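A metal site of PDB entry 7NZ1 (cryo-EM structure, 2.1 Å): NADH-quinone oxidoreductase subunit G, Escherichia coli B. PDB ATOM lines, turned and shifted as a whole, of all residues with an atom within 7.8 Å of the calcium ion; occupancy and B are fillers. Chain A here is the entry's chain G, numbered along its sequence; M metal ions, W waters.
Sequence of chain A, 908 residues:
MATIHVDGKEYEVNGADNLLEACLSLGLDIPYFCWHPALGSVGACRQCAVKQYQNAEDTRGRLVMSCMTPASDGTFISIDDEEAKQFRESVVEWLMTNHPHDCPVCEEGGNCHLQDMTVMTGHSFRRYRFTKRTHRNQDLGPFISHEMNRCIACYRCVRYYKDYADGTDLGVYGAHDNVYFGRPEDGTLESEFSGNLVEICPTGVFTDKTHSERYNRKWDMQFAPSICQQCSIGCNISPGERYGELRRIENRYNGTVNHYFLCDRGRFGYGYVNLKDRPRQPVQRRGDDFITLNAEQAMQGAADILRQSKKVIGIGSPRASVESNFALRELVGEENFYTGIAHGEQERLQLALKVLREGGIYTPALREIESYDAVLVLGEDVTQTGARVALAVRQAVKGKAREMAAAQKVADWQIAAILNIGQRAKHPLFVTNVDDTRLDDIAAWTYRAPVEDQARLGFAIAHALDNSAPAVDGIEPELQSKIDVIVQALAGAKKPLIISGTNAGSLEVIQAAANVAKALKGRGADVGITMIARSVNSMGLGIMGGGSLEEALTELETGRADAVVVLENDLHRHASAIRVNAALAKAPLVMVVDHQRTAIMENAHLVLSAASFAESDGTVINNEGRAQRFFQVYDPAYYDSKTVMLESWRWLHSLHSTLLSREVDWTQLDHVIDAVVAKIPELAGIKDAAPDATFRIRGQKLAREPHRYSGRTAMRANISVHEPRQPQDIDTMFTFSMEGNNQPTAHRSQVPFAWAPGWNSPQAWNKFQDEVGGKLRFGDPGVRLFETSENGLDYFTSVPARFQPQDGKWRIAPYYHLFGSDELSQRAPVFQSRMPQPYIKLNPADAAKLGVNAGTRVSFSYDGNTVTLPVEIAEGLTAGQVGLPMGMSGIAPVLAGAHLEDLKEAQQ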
ATOM      1  N   GLU A 615     -14.294  19.018  -9.220  1.00  0.00           N
ATOM      2  CA  GLU A 615     -13.688  20.345  -9.296  1.00  0.00           C
ATOM      3  C   GLU A 615     -14.347  21.349  -8.358  1.00  0.00           C
ATOM      4  O   GLU A 615     -14.127  22.551  -8.502  1.00  0.00           O
ATOM      5  CB  GLU A 615     -13.738  20.868 -10.734  1.00  0.00           C
ATOM      6  CG  GLU A 615     -13.142  19.933 -11.776  1.00  0.00           C
ATOM      7  CD  GLU A 615     -14.184  19.181 -12.586  1.00  0.00           C
ATOM      8  OE1 GLU A 615     -14.681  18.143 -12.126  1.00  0.00           O
ATOM      9  OE2 GLU A 615     -14.487  19.624 -13.716  1.00  0.00           O
ATOM     10  N   SER A 616     -15.138  20.895  -7.394  1.00  0.00           N
ATOM     11  CA  SER A 616     -15.927  21.796  -6.557  1.00  0.00           C
ATOM     12  C   SER A 616     -15.852  21.384  -5.099  1.00  0.00           C
ATOM     13  O   SER A 616     -15.378  20.310  -4.749  1.00  0.00           O
ATOM     14  CB  SER A 616     -17.395  21.836  -7.017  1.00  0.00           C
ATOM     15  OG  SER A 616     -18.199  22.592  -6.129  1.00  0.00           O
ATOM     16  N   ASP A 617     -16.393  22.258  -4.260  1.00  0.00           N
ATOM     17  CA  ASP A 617     -16.541  22.046  -2.838  1.00  0.00           C
ATOM     18  C   ASP A 617     -17.995  22.303  -2.482  1.00  0.00           C
ATOM     19  O   ASP A 617     -18.724  22.940  -3.253  1.00  0.00           O
ATOM     20  CB  ASP A 617     -15.636  22.980  -2.012  1.00  0.00           C
ATOM     21  CG  ASP A 617     -14.189  22.922  -2.432  1.00  0.00           C
ATOM     22  OD1 ASP A 617     -13.532  21.896  -2.179  1.00  0.00           O
ATOM     23  OD2 ASP A 617     -13.702  23.916  -2.996  1.00  0.00           O
ATOM     24  N   GLY A 618     -18.408  21.850  -1.320  1.00  0.00           N
ATOM     25  CA  GLY A 618     -19.814  21.945  -0.980  1.00  0.00           C
ATOM     26  C   GLY A 618     -20.231  20.876   0.012  1.00  0.00           C
ATOM     27  O   GLY A 618     -19.465  19.992   0.377  1.00  0.00           O
ATOM     28  N   PHE A 631     -14.697  17.784  -0.916  1.00  0.00           N
ATOM     29  CA  PHE A 631     -13.602  18.698  -1.184  1.00  0.00           C
ATOM     30  C   PHE A 631     -13.179  18.583  -2.639  1.00  0.00           C
ATOM     31  O   PHE A 631     -13.368  17.548  -3.274  1.00  0.00           O
ATOM     32  CB  PHE A 631     -12.419  18.411  -0.246  1.00  0.00           C
ATOM     33  CG  PHE A 631     -12.748  18.566   1.230  1.00  0.00           C
ATOM     34  CD1 PHE A 631     -13.305  17.510   1.960  1.00  0.00           C
ATOM     35  CD2 PHE A 631     -12.515  19.766   1.885  1.00  0.00           C
ATOM     36  CE1 PHE A 631     -13.622  17.666   3.309  1.00  0.00           C
ATOM     37  CE2 PHE A 631     -12.816  19.916   3.229  1.00  0.00           C
ATOM     38  CZ  PHE A 631     -13.367  18.873   3.941  1.00  0.00           C
ATOM     39  N   GLN A 632     -12.609  19.675  -3.161  1.00  0.00           N
ATOM     40  CA  GLN A 632     -12.113  19.707  -4.525  1.00  0.00           C
ATOM     41  C   GLN A 632     -10.896  18.800  -4.697  1.00  0.00           C
ATOM     42  O   GLN A 632      -9.982  18.806  -3.875  1.00  0.00           O
ATOM     43  CB  GLN A 632     -11.791  21.155  -4.904  1.00  0.00           C
ATOM     44  CG  GLN A 632     -11.298  21.392  -6.286  1.00  0.00           C
ATOM     45  CD  GLN A 632     -11.282  22.860  -6.635  1.00  0.00           C
ATOM     46  OE1 GLN A 632     -12.068  23.650  -6.107  1.00  0.00           O
ATOM     47  NE2 GLN A 632     -10.392  23.254  -7.533  1.00  0.00           N
ATOM     48  N   VAL A 633     -10.885  18.045  -5.794  1.00  0.00           N
ATOM     49  CA  VAL A 633      -9.764  17.152  -6.087  1.00  0.00           C
ATOM     50  C   VAL A 633      -8.615  17.888  -6.769  1.00  0.00           C
ATOM     51  O   VAL A 633      -7.456  17.739  -6.398  1.00  0.00           O
ATOM     52  CB  VAL A 633     -10.241  15.960  -6.934  1.00  0.00           C
ATOM     53  CG1 VAL A 633      -9.134  14.930  -7.079  1.00  0.00           C
ATOM     54  CG2 VAL A 633     -11.436  15.347  -6.287  1.00  0.00           C
ATOM     55  N   TYR A 634      -8.932  18.703  -7.768  1.00  0.00           N
ATOM     56  CA  TYR A 634      -7.881  19.285  -8.595  1.00  0.00           C
ATOM     57  C   TYR A 634      -8.362  20.609  -9.161  1.00  0.00           C
ATOM     58  O   TYR A 634      -9.563  20.861  -9.296  1.00  0.00           O
ATOM     59  CB  TYR A 634      -7.472  18.338  -9.727  1.00  0.00           C
ATOM     60  CG  TYR A 634      -8.518  18.205 -10.836  1.00  0.00           C
ATOM     61  CD1 TYR A 634      -9.658  17.421 -10.649  1.00  0.00           C
ATOM     62  CD2 TYR A 634      -8.356  18.862 -12.047  1.00  0.00           C
ATOM     63  CE1 TYR A 634     -10.603  17.304 -11.643  1.00  0.00           C
ATOM     64  CE2 TYR A 634      -9.310  18.756 -13.041  1.00  0.00           C
ATOM     65  CZ  TYR A 634     -10.422  17.968 -12.841  1.00  0.00           C
ATOM     66  OH  TYR A 634     -11.375  17.855 -13.824  1.00  0.00           O
ATOM     67  N   LEU A 646     -15.675  27.452 -12.455  1.00  0.00           N
ATOM     68  CA  LEU A 646     -15.862  27.824 -11.066  1.00  0.00           C
ATOM     69  C   LEU A 646     -17.017  27.051 -10.458  1.00  0.00           C
ATOM     70  O   LEU A 646     -17.829  26.454 -11.162  1.00  0.00           O
ATOM     71  CB  LEU A 646     -16.111  29.326 -10.915  1.00  0.00           C
ATOM     72  CG  LEU A 646     -15.301  30.274 -11.795  1.00  0.00           C
ATOM     73  CD1 LEU A 646     -15.853  31.658 -11.662  1.00  0.00           C
ATOM     74  CD2 LEU A 646     -13.838  30.242 -11.423  1.00  0.00           C
ATOM     75  N   GLU A 647     -17.048  27.036  -9.117  1.00  0.00           N
ATOM     76  CA  GLU A 647     -18.168  26.463  -8.381  1.00  0.00           C
ATOM     77  C   GLU A 647     -19.458  27.202  -8.692  1.00  0.00           C
ATOM     78  O   GLU A 647     -19.456  28.388  -9.021  1.00  0.00           O
ATOM     79  CB  GLU A 647     -17.894  26.506  -6.875  1.00  0.00           C
ATOM     80  CG  GLU A 647     -16.776  25.586  -6.410  1.00  0.00           C
ATOM     81  CD  GLU A 647     -15.432  26.264  -6.323  1.00  0.00           C
ATOM     82  OE1 GLU A 647     -15.052  26.999  -7.259  1.00  0.00           O
ATOM     83  OE2 GLU A 647     -14.734  26.075  -5.303  1.00  0.00           O
ATOM     84  N   TRP A 649     -21.865  27.891  -6.555  1.00  0.00           N
ATOM     85  CA  TRP A 649     -22.059  28.913  -5.530  1.00  0.00           C
ATOM     86  C   TRP A 649     -21.147  30.119  -5.760  1.00  0.00           C
ATOM     87  O   TRP A 649     -21.504  31.233  -5.382  1.00  0.00           O
ATOM     88  CB  TRP A 649     -21.872  28.313  -4.140  1.00  0.00           C
ATOM     89  CG  TRP A 649     -20.547  27.643  -3.887  1.00  0.00           C
ATOM     90  CD1 TRP A 649     -20.301  26.311  -3.928  1.00  0.00           C
ATOM     91  CD2 TRP A 649     -19.317  28.272  -3.480  1.00  0.00           C
ATOM     92  NE1 TRP A 649     -18.981  26.069  -3.626  1.00  0.00           N
ATOM     93  CE2 TRP A 649     -18.354  27.248  -3.344  1.00  0.00           C
ATOM     94  CE3 TRP A 649     -18.933  29.590  -3.238  1.00  0.00           C
ATOM     95  CZ2 TRP A 649     -17.043  27.503  -2.972  1.00  0.00           C
ATOM     96  CZ3 TRP A 649     -17.629  29.855  -2.884  1.00  0.00           C
ATOM     97  CH2 TRP A 649     -16.699  28.813  -2.749  1.00  0.00           C
ATOM     98  N   ARG A 650     -19.955  29.907  -6.333  1.00  0.00           N
ATOM     99  CA  ARG A 650     -19.065  31.029  -6.608  1.00  0.00           C
ATOM    100  C   ARG A 650     -19.576  31.856  -7.790  1.00  0.00           C
ATOM    101  O   ARG A 650     -19.438  33.085  -7.778  1.00  0.00           O
ATOM    102  CB  ARG A 650     -17.631  30.531  -6.806  1.00  0.00           C
ATOM    103  CG  ARG A 650     -16.614  31.604  -7.153  1.00  0.00           C
ATOM    104  CD  ARG A 650     -15.138  31.192  -7.011  1.00  0.00           C
ATOM    105  NE  ARG A 650     -14.628  31.377  -5.654  1.00  0.00           N
ATOM    106  CZ  ARG A 650     -14.349  30.392  -4.814  1.00  0.00           C
ATOM    107  NH1 ARG A 650     -14.457  29.125  -5.165  1.00  0.00           N
ATOM    108  NH2 ARG A 650     -13.930  30.694  -3.588  1.00  0.00           N
ATOM    109  N   LEU A 669     -15.597  29.827   0.629  1.00  0.00           N
ATOM    110  CA  LEU A 669     -16.598  28.809   0.935  1.00  0.00           C
ATOM    111  C   LEU A 669     -17.188  28.957   2.329  1.00  0.00           C
ATOM    112  O   LEU A 669     -18.394  28.737   2.505  1.00  0.00           O
ATOM    113  CB  LEU A 669     -15.985  27.408   0.771  1.00  0.00           C
ATOM    114  CG  LEU A 669     -16.883  26.214   1.135  1.00  0.00           C
ATOM    115  CD1 LEU A 669     -18.143  26.183   0.290  1.00  0.00           C
ATOM    116  CD2 LEU A 669     -16.158  24.893   1.084  1.00  0.00           C
ATOM    117  N   ARG A 704      -3.030  16.689  -0.227  1.00  0.00           N
ATOM    118  CA  ARG A 704      -3.803  15.974  -1.238  1.00  0.00           C
ATOM    119  C   ARG A 704      -2.987  14.912  -1.969  1.00  0.00           C
ATOM    120  O   ARG A 704      -3.549  13.933  -2.446  1.00  0.00           O
ATOM    121  CB  ARG A 704      -4.363  16.935  -2.288  1.00  0.00           C
ATOM    122  CG  ARG A 704      -5.588  17.727  -1.869  1.00  0.00           C
ATOM    123  CD  ARG A 704      -6.117  18.493  -3.074  1.00  0.00           C
ATOM    124  NE  ARG A 704      -7.415  19.113  -2.821  1.00  0.00           N
ATOM    125  CZ  ARG A 704      -7.579  20.359  -2.385  1.00  0.00           C
ATOM    126  NH1 ARG A 704      -6.546  21.145  -2.126  1.00  0.00           N
ATOM    127  NH2 ARG A 704      -8.814  20.825  -2.210  1.00  0.00           N
ATOM    128  N   GLN A 728      -3.459  27.483  -5.215  1.00  0.00           N
ATOM    129  CA  GLN A 728      -3.685  27.878  -3.835  1.00  0.00           C
ATOM    130  C   GLN A 728      -5.161  27.688  -3.506  1.00  0.00           C
ATOM    131  O   GLN A 728      -6.032  28.122  -4.266  1.00  0.00           O
ATOM    132  CB  GLN A 728      -3.280  29.339  -3.602  1.00  0.00           C
ATOM    133  CG  GLN A 728      -1.784  29.563  -3.555  1.00  0.00           C
ATOM    134  CD  GLN A 728      -1.124  28.968  -2.333  1.00  0.00           C
ATOM    135  OE1 GLN A 728      -0.432  27.955  -2.419  1.00  0.00           O
ATOM    136  NE2 GLN A 728      -1.326  29.592  -1.184  1.00  0.00           N
ATOM    137  N   ASP A 729      -5.427  27.033  -2.381  1.00  0.00           N
ATOM    138  CA  ASP A 729      -6.780  26.722  -1.961  1.00  0.00           C
ATOM    139  C   ASP A 729      -7.146  27.607  -0.778  1.00  0.00           C
ATOM    140  O   ASP A 729      -6.530  27.519   0.287  1.00  0.00           O
ATOM    141  CB  ASP A 729      -6.919  25.248  -1.583  1.00  0.00           C
ATOM    142  CG  ASP A 729      -8.363  24.802  -1.389  1.00  0.00           C
ATOM    143  OD1 ASP A 729      -9.304  25.588  -1.655  1.00  0.00           O
ATOM    144  OD2 ASP A 729      -8.576  23.647  -0.945  1.00  0.00           O
ATOM    145  N   ILE A 730      -8.138  28.467  -0.968  1.00  0.00           N
ATOM    146  CA  ILE A 730      -8.588  29.384   0.071  1.00  0.00           C
ATOM    147  C   ILE A 730      -9.897  28.921   0.661  1.00  0.00           C
ATOM    148  O   ILE A 730     -10.316  29.454   1.703  1.00  0.00           O
ATOM    149  CB  ILE A 730      -8.691  30.843  -0.446  1.00  0.00           C
ATOM    150  CG1 ILE A 730      -9.218  30.929  -1.888  1.00  0.00           C
ATOM    151  CG2 ILE A 730      -7.361  31.558  -0.326  1.00  0.00           C
ATOM    152  CD1 ILE A 730     -10.728  30.883  -2.063  1.00  0.00           C
ATOM    153  N   ASP A 731     -10.529  27.914   0.060  1.00  0.00           N
ATOM    154  CA  ASP A 731     -11.831  27.416   0.466  1.00  0.00           C
ATOM    155  C   ASP A 731     -11.726  26.404   1.593  1.00  0.00           C
ATOM    156  O   ASP A 731     -12.534  26.434   2.533  1.00  0.00           O
ATOM    157  CB  ASP A 731     -12.502  26.750  -0.738  1.00  0.00           C
ATOM    158  CG  ASP A 731     -13.063  27.750  -1.738  1.00  0.00           C
ATOM    159  OD1 ASP A 731     -13.616  28.782  -1.309  1.00  0.00           O
ATOM    160  OD2 ASP A 731     -12.923  27.490  -2.942  1.00  0.00           O
ATOM    161  N   THR A 732     -10.744  25.507   1.524  1.00  0.00           N
ATOM    162  CA  THR A 732     -10.638  24.370   2.435  1.00  0.00           C
ATOM    163  C   THR A 732      -9.255  24.320   3.070  1.00  0.00           C
ATOM    164  O   THR A 732      -8.321  25.015   2.684  1.00  0.00           O
ATOM    165  CB  THR A 732     -10.888  23.017   1.733  1.00  0.00           C
ATOM    166  OG1 THR A 732      -9.633  22.516   1.231  1.00  0.00           O
ATOM    167  CG2 THR A 732     -11.879  23.105   0.579  1.00  0.00           C
ATOM    168  N   PHE A 736      -3.147  22.004  -2.615  1.00  0.00           N
ATOM    169  CA  PHE A 736      -2.976  21.344  -3.920  1.00  0.00           C
ATOM    170  C   PHE A 736      -1.517  20.926  -4.160  1.00  0.00           C
ATOM    171  O   PHE A 736      -0.929  21.231  -5.192  1.00  0.00           O
ATOM    172  CB  PHE A 736      -3.434  22.273  -5.039  1.00  0.00           C
ATOM    173  CG  PHE A 736      -4.912  22.412  -5.156  1.00  0.00           C
ATOM    174  CD1 PHE A 736      -5.673  21.395  -5.705  1.00  0.00           C
ATOM    175  CD2 PHE A 736      -5.542  23.572  -4.741  1.00  0.00           C
ATOM    176  CE1 PHE A 736      -7.036  21.528  -5.815  1.00  0.00           C
ATOM    177  CE2 PHE A 736      -6.912  23.707  -4.857  1.00  0.00           C
ATOM    178  CZ  PHE A 736      -7.659  22.685  -5.394  1.00  0.00           C
HETATM  179 CA    CA M   1     -12.540  25.486  -4.446  1.00  0.00          CA
HETATM  180  O   HOH W   1     -11.332  27.120  -6.017  1.00  0.00           O
HETATM  181  O   HOH W   2      -9.699  25.620  -4.505  1.00  0.00           O
HETATM  182  O   HOH W   3     -10.968  23.541  -2.755  1.00  0.00           O
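The side-chain carboxylate of Glu 647 lies within salt-bridge range of the guanidinium group of Arg 650 (3.0 Å).
The side-chain amide oxygen of Gln 632 sits close to the backbone carbonyl oxygen of Glu 615.
N of Gln 632 is in hydrogen-bond range of O of Ser 616, at 3.3 Å.
The guanidinium group of Arg 704 sits at hydrogen-bond distance from the backbone carbonyl oxygen of Gln 632 (2.8 Å).
O of Tyr 634 lies within hydrogen-bond range of NE2 of Gln 632.
The guanidinium group (NH2) of Arg 650 is in salt-bridge range of the side-chain carboxylate (OD1) of Asp 731 (3.0 Å).
The backbone NH (N) of Asp 731 sits at hydrogen-bond distance from the side-chain carboxylate (OD1) of Asp 729 (3.1 Å).
The side-chain carboxylate (OD1) of Asp 731 sits at hydrogen-bond distance from the backbone NH (N) of Leu 669, 3.0 Å away.
Within 4 Å of the calcium ion: Asp 617, Gln 632, Glu 647 and Asp 731.
The nearest printed residue that does not touch the calcium ion is Arg 650 (4.2 Å).
The calcium ion is bound by the side-chain carboxylate of Glu 647, the side-chain carboxylate of Asp 617, the side-chain amide oxygen of Gln 632, the side-chain carboxylate of Asp 731, water W1 and water W2.
Slightly farther from the calcium ion lies water W3 (3.0 Å).
Water W3 bridges OD1 of Asp 729 (2.9 Å) and OD1 of Asp 617 (3.1 Å).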
